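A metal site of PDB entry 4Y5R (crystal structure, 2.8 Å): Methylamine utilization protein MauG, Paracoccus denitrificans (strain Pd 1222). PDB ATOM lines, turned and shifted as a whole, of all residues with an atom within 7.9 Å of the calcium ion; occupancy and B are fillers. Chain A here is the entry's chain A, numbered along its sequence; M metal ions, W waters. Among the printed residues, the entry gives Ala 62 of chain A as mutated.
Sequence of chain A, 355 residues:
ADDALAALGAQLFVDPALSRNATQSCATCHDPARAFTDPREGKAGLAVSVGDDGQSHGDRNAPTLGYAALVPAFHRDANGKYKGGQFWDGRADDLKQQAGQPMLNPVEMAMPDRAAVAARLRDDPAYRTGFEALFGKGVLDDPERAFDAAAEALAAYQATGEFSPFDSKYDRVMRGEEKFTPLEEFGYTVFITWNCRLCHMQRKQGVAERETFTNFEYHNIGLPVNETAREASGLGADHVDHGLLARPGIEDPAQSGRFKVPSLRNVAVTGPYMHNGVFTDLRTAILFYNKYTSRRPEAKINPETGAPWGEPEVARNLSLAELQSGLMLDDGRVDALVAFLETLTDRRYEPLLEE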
ATOM      1  N   ARG A  34     -29.037 -19.845  17.141  1.00  0.00           N
ATOM      2  CA  ARG A  34     -27.564 -19.762  17.284  1.00  0.00           C
ATOM      3  C   ARG A  34     -26.874 -19.047  16.110  1.00  0.00           C
ATOM      4  O   ARG A  34     -25.906 -19.538  15.531  1.00  0.00           O
ATOM      5  CB  ARG A  34     -26.945 -21.147  17.588  1.00  0.00           C
ATOM      6  CG  ARG A  34     -25.873 -21.026  18.649  1.00  0.00           C
ATOM      7  CD  ARG A  34     -25.099 -22.297  18.859  1.00  0.00           C
ATOM      8  NE  ARG A  34     -24.125 -22.499  17.787  1.00  0.00           N
ATOM      9  CZ  ARG A  34     -22.810 -22.674  17.934  1.00  0.00           C
ATOM     10  NH1 ARG A  34     -22.225 -22.720  19.120  1.00  0.00           N
ATOM     11  NH2 ARG A  34     -22.080 -22.835  16.847  1.00  0.00           N
ATOM     12  N   THR A  37     -26.146 -20.908  12.742  1.00  0.00           N
ATOM     13  CA  THR A  37     -25.172 -21.984  12.648  1.00  0.00           C
ATOM     14  C   THR A  37     -25.738 -23.253  13.288  1.00  0.00           C
ATOM     15  O   THR A  37     -26.891 -23.249  13.744  1.00  0.00           O
ATOM     16  CB  THR A  37     -23.840 -21.619  13.321  1.00  0.00           C
ATOM     17  OG1 THR A  37     -24.019 -21.603  14.739  1.00  0.00           O
ATOM     18  CG2 THR A  37     -23.348 -20.269  12.842  1.00  0.00           C
ATOM     19  N   ASP A  38     -24.932 -24.311  13.305  1.00  0.00           N
ATOM     20  CA  ASP A  38     -25.357 -25.666  13.709  1.00  0.00           C
ATOM     21  C   ASP A  38     -25.035 -25.971  15.198  1.00  0.00           C
ATOM     22  O   ASP A  38     -23.862 -26.186  15.567  1.00  0.00           O
ATOM     23  CB  ASP A  38     -24.677 -26.692  12.766  1.00  0.00           C
ATOM     24  CG  ASP A  38     -25.309 -28.087  12.832  1.00  0.00           C
ATOM     25  OD1 ASP A  38     -26.278 -28.325  13.601  1.00  0.00           O
ATOM     26  OD2 ASP A  38     -24.822 -28.959  12.080  1.00  0.00           O
ATOM     27  N   LEU A  46     -19.048 -30.128  17.212  1.00  0.00           N
ATOM     28  CA  LEU A  46     -19.765 -29.194  16.351  1.00  0.00           C
ATOM     29  C   LEU A  46     -18.887 -28.732  15.191  1.00  0.00           C
ATOM     30  O   LEU A  46     -19.290 -27.807  14.452  1.00  0.00           O
ATOM     31  CB  LEU A  46     -20.225 -27.959  17.155  1.00  0.00           C
ATOM     32  CG  LEU A  46     -21.657 -27.877  17.667  1.00  0.00           C
ATOM     33  CD1 LEU A  46     -21.923 -28.973  18.669  1.00  0.00           C
ATOM     34  CD2 LEU A  46     -21.888 -26.523  18.324  1.00  0.00           C
ATOM     35  N   ALA A  47     -17.697 -29.335  15.032  1.00  0.00           N
ATOM     36  CA  ALA A  47     -16.782 -28.931  13.951  1.00  0.00           C
ATOM     37  C   ALA A  47     -17.451 -29.030  12.555  1.00  0.00           C
ATOM     38  O   ALA A  47     -17.311 -28.115  11.754  1.00  0.00           O
ATOM     39  CB  ALA A  47     -15.494 -29.729  14.004  1.00  0.00           C
ATOM     40  N   ASN A  61     -16.906 -26.538   8.548  1.00  0.00           N
ATOM     41  CA  ASN A  61     -17.799 -25.862   9.488  1.00  0.00           C
ATOM     42  C   ASN A  61     -18.851 -25.040   8.728  1.00  0.00           C
ATOM     43  O   ASN A  61     -18.583 -24.399   7.695  1.00  0.00           O
ATOM     44  CB  ASN A  61     -16.996 -24.967  10.428  1.00  0.00           C
ATOM     45  CG  ASN A  61     -17.818 -24.436  11.603  1.00  0.00           C
ATOM     46  OD1 ASN A  61     -18.163 -23.251  11.658  1.00  0.00           O
ATOM     47  ND2 ASN A  61     -18.100 -25.319  12.587  1.00  0.00           N
ATOM     48  N   ALA A  62     -20.065 -25.112   9.242  1.00  0.00           N
ATOM     49  CA  ALA A  62     -21.167 -24.385   8.699  1.00  0.00           C
ATOM     50  C   ALA A  62     -21.095 -22.941   9.202  1.00  0.00           C
ATOM     51  O   ALA A  62     -21.256 -22.669  10.405  1.00  0.00           O
ATOM     52  CB  ALA A  62     -22.454 -25.035   9.140  1.00  0.00           C
ATOM     53  N   PRO A  63     -20.848 -21.992   8.303  1.00  0.00           N
ATOM     54  CA  PRO A  63     -20.801 -20.595   8.736  1.00  0.00           C
ATOM     55  C   PRO A  63     -22.172 -19.971   9.068  1.00  0.00           C
ATOM     56  O   PRO A  63     -23.229 -20.545   8.803  1.00  0.00           O
ATOM     57  CB  PRO A  63     -20.177 -19.898   7.539  1.00  0.00           C
ATOM     58  CG  PRO A  63     -20.617 -20.727   6.397  1.00  0.00           C
ATOM     59  CD  PRO A  63     -20.597 -22.131   6.869  1.00  0.00           C
ATOM     60  N   THR A  64     -22.126 -18.783   9.673  1.00  0.00           N
ATOM     61  CA  THR A  64     -23.294 -17.959   9.836  1.00  0.00           C
ATOM     62  C   THR A  64     -23.822 -17.583   8.448  1.00  0.00           C
ATOM     63  O   THR A  64     -23.046 -17.507   7.480  1.00  0.00           O
ATOM     64  CB  THR A  64     -22.995 -16.662  10.628  1.00  0.00           C
ATOM     65  OG1 THR A  64     -24.182 -15.871  10.764  1.00  0.00           O
ATOM     66  CG2 THR A  64     -21.947 -15.801   9.931  1.00  0.00           C
ATOM     67  N   TRP A  88     -16.832 -21.297   1.936  1.00  0.00           N
ATOM     68  CA  TRP A  88     -15.462 -20.964   2.408  1.00  0.00           C
ATOM     69  C   TRP A  88     -14.471 -20.915   1.243  1.00  0.00           C
ATOM     70  O   TRP A  88     -13.432 -20.274   1.370  1.00  0.00           O
ATOM     71  CB  TRP A  88     -14.904 -21.978   3.452  1.00  0.00           C
ATOM     72  CG  TRP A  88     -15.575 -22.031   4.830  1.00  0.00           C
ATOM     73  CD1 TRP A  88     -16.544 -22.909   5.225  1.00  0.00           C
ATOM     74  CD2 TRP A  88     -15.277 -21.220   5.984  1.00  0.00           C
ATOM     75  NE1 TRP A  88     -16.884 -22.679   6.548  1.00  0.00           N
ATOM     76  CE2 TRP A  88     -16.130 -21.649   7.027  1.00  0.00           C
ATOM     77  CE3 TRP A  88     -14.389 -20.158   6.220  1.00  0.00           C
ATOM     78  CZ2 TRP A  88     -16.123 -21.056   8.299  1.00  0.00           C
ATOM     79  CZ3 TRP A  88     -14.379 -19.574   7.490  1.00  0.00           C
ATOM     80  CH2 TRP A  88     -15.242 -20.034   8.507  1.00  0.00           C
ATOM     81  N   VAL A 267     -19.062 -13.398  16.098  1.00  0.00           N
ATOM     82  CA  VAL A 267     -18.029 -14.419  16.196  1.00  0.00           C
ATOM     83  C   VAL A 267     -18.065 -15.159  17.549  1.00  0.00           C
ATOM     84  O   VAL A 267     -18.014 -16.390  17.606  1.00  0.00           O
ATOM     85  CB  VAL A 267     -16.618 -13.870  15.864  1.00  0.00           C
ATOM     86  CG1 VAL A 267     -16.122 -12.881  16.894  1.00  0.00           C
ATOM     87  CG2 VAL A 267     -15.624 -15.006  15.736  1.00  0.00           C
ATOM     88  N   VAL A 269     -20.420 -16.180  19.236  1.00  0.00           N
ATOM     89  CA  VAL A 269     -21.450 -17.201  19.400  1.00  0.00           C
ATOM     90  C   VAL A 269     -21.468 -18.266  18.308  1.00  0.00           C
ATOM     91  O   VAL A 269     -22.391 -19.077  18.256  1.00  0.00           O
ATOM     92  CB  VAL A 269     -22.860 -16.577  19.621  1.00  0.00           C
ATOM     93  CG1 VAL A 269     -22.809 -15.589  20.768  1.00  0.00           C
ATOM     94  CG2 VAL A 269     -23.386 -15.868  18.393  1.00  0.00           C
ATOM     95  N   THR A 270     -20.425 -18.314  17.480  1.00  0.00           N
ATOM     96  CA  THR A 270     -20.441 -19.211  16.310  1.00  0.00           C
ATOM     97  C   THR A 270     -19.324 -20.251  16.279  1.00  0.00           C
ATOM     98  O   THR A 270     -19.036 -20.802  15.220  1.00  0.00           O
ATOM     99  CB  THR A 270     -20.486 -18.419  14.991  1.00  0.00           C
ATOM    100  OG1 THR A 270     -19.325 -17.580  14.877  1.00  0.00           O
ATOM    101  CG2 THR A 270     -21.765 -17.554  14.940  1.00  0.00           C
ATOM    102  N   GLY A 271     -18.742 -20.542  17.447  1.00  0.00           N
ATOM    103  CA  GLY A 271     -17.664 -21.541  17.558  1.00  0.00           C
ATOM    104  C   GLY A 271     -18.211 -22.949  17.415  1.00  0.00           C
ATOM    105  O   GLY A 271     -19.392 -23.166  17.705  1.00  0.00           O
ATOM    106  N   PRO A 272     -17.371 -23.940  17.015  1.00  0.00           N
ATOM    107  CA  PRO A 272     -15.921 -23.848  16.824  1.00  0.00           C
ATOM    108  C   PRO A 272     -15.517 -23.057  15.603  1.00  0.00           C
ATOM    109  O   PRO A 272     -16.361 -22.704  14.742  1.00  0.00           O
ATOM    110  CB  PRO A 272     -15.494 -25.309  16.680  1.00  0.00           C
ATOM    111  CG  PRO A 272     -16.668 -25.975  16.104  1.00  0.00           C
ATOM    112  CD  PRO A 272     -17.843 -25.308  16.745  1.00  0.00           C
ATOM    113  N   TYR A 273     -14.222 -22.762  15.529  1.00  0.00           N
ATOM    114  CA  TYR A 273     -13.747 -21.767  14.622  1.00  0.00           C
ATOM    115  C   TYR A 273     -12.966 -22.331  13.432  1.00  0.00           C
ATOM    116  O   TYR A 273     -12.472 -23.467  13.484  1.00  0.00           O
ATOM    117  CB  TYR A 273     -12.945 -20.722  15.409  1.00  0.00           C
ATOM    118  CG  TYR A 273     -13.821 -19.970  16.374  1.00  0.00           C
ATOM    119  CD1 TYR A 273     -14.854 -19.142  15.920  1.00  0.00           C
ATOM    120  CD2 TYR A 273     -13.644 -20.106  17.749  1.00  0.00           C
ATOM    121  CE1 TYR A 273     -15.688 -18.478  16.805  1.00  0.00           C
ATOM    122  CE2 TYR A 273     -14.472 -19.432  18.646  1.00  0.00           C
ATOM    123  CZ  TYR A 273     -15.489 -18.615  18.169  1.00  0.00           C
ATOM    124  OH  TYR A 273     -16.292 -17.952  19.053  1.00  0.00           O
ATOM    125  N   MET A 274     -12.921 -21.521  12.369  1.00  0.00           N
ATOM    126  CA  MET A 274     -12.214 -21.785  11.120  1.00  0.00           C
ATOM    127  C   MET A 274     -13.009 -22.745  10.248  1.00  0.00           C
ATOM    128  O   MET A 274     -13.982 -23.330  10.723  1.00  0.00           O
ATOM    129  CB  MET A 274     -10.791 -22.304  11.337  1.00  0.00           C
ATOM    130  CG  MET A 274      -9.894 -21.434  12.239  1.00  0.00           C
ATOM    131  SD  MET A 274      -9.701 -19.683  11.789  1.00  0.00           S
ATOM    132  CE  MET A 274      -8.552 -19.136  13.036  1.00  0.00           C
ATOM    133  N   HIS A 275     -12.585 -22.884   8.982  1.00  0.00           N
ATOM    134  CA  HIS A 275     -13.296 -23.667   7.959  1.00  0.00           C
ATOM    135  C   HIS A 275     -13.523 -25.141   8.323  1.00  0.00           C
ATOM    136  O   HIS A 275     -14.436 -25.776   7.806  1.00  0.00           O
ATOM    137  CB  HIS A 275     -12.607 -23.542   6.574  1.00  0.00           C
ATOM    138  CG  HIS A 275     -11.304 -24.269   6.468  1.00  0.00           C
ATOM    139  ND1 HIS A 275     -10.085 -23.621   6.488  1.00  0.00           N
ATOM    140  CD2 HIS A 275     -11.019 -25.585   6.327  1.00  0.00           C
ATOM    141  CE1 HIS A 275      -9.111 -24.503   6.392  1.00  0.00           C
ATOM    142  NE2 HIS A 275      -9.654 -25.704   6.290  1.00  0.00           N
ATOM    143  N   ASN A 276     -12.701 -25.661   9.223  1.00  0.00           N
ATOM    144  CA  ASN A 276     -12.742 -27.067   9.656  1.00  0.00           C
ATOM    145  C   ASN A 276     -12.959 -27.234  11.170  1.00  0.00           C
ATOM    146  O   ASN A 276     -12.492 -28.213  11.754  1.00  0.00           O
ATOM    147  CB  ASN A 276     -11.424 -27.776   9.236  1.00  0.00           C
ATOM    148  CG  ASN A 276     -10.207 -27.264   9.994  1.00  0.00           C
ATOM    149  OD1 ASN A 276     -10.302 -26.485  10.940  1.00  0.00           O
ATOM    150  ND2 ASN A 276      -9.047 -27.713   9.571  1.00  0.00           N
ATOM    151  N   GLY A 277     -13.644 -26.259  11.786  1.00  0.00           N
ATOM    152  CA  GLY A 277     -13.952 -26.266  13.213  1.00  0.00           C
ATOM    153  C   GLY A 277     -12.850 -26.775  14.147  1.00  0.00           C
ATOM    154  O   GLY A 277     -13.150 -27.412  15.161  1.00  0.00           O
ATOM    155  N   PHE A 279     -10.695 -25.297  16.182  1.00  0.00           N
ATOM    156  CA  PHE A 279     -10.614 -24.645  17.494  1.00  0.00           C
ATOM    157  C   PHE A 279     -11.977 -24.332  18.090  1.00  0.00           C
ATOM    158  O   PHE A 279     -12.820 -23.711  17.436  1.00  0.00           O
ATOM    159  CB  PHE A 279      -9.894 -23.320  17.391  1.00  0.00           C
ATOM    160  CG  PHE A 279      -8.566 -23.389  16.702  1.00  0.00           C
ATOM    161  CD1 PHE A 279      -7.638 -24.366  17.037  1.00  0.00           C
ATOM    162  CD2 PHE A 279      -8.212 -22.438  15.759  1.00  0.00           C
ATOM    163  CE1 PHE A 279      -6.412 -24.417  16.405  1.00  0.00           C
ATOM    164  CE2 PHE A 279      -6.986 -22.486  15.118  1.00  0.00           C
ATOM    165  CZ  PHE A 279      -6.075 -23.477  15.441  1.00  0.00           C
HETATM  166 CA    CA M   1     -18.095 -21.717  13.301  1.00  0.00          CA
HETATM  167  O   HOH W   1     -16.302 -21.278  11.404  1.00  0.00           O
HETATM  168  O   HOH W   2     -19.082 -23.388  14.364  1.00  0.00           O
HETATM  169  O   HOH W   3     -17.427 -19.478  14.027  1.00  0.00           O
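The calcium ion is bound by water W2 (2.2 Å), OD1 of Asn 61 (2.2 Å), O of Thr 270 (2.3 Å), water W3 (2.4 Å), O of Pro 272 (2.5 Å) and water W1 (2.6 Å).
Within 4 Å of the calcium ion: Asn 61, Thr 270 and Pro 272.
The indole nitrogen (NE1) of Trp 88 lies within hydrogen-bond range of the backbone carbonyl oxygen (O) of Asn 61 (2.7 Å). The backbone carbonyl oxygen (O) of Leu 46 is in hydrogen-bond range of the side-chain amide nitrogen (ND2) of Asn 61, at 3.3 Å. The backbone carbonyl oxygen (O) of Ala 47 is in hydrogen-bond range of the side-chain amide nitrogen (ND2) of Asn 61 (3.0 Å). The backbone NH of Asn 61 sits at hydrogen-bond distance from the backbone carbonyl oxygen of His 275. The side-chain hydroxyl (OG1) of Thr 270 sits at hydrogen-bond distance from the backbone carbonyl oxygen (O) of Val 267 (3.3 Å).
Water W2 bridges ND2 of Asn 61 and O of Gly 271.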
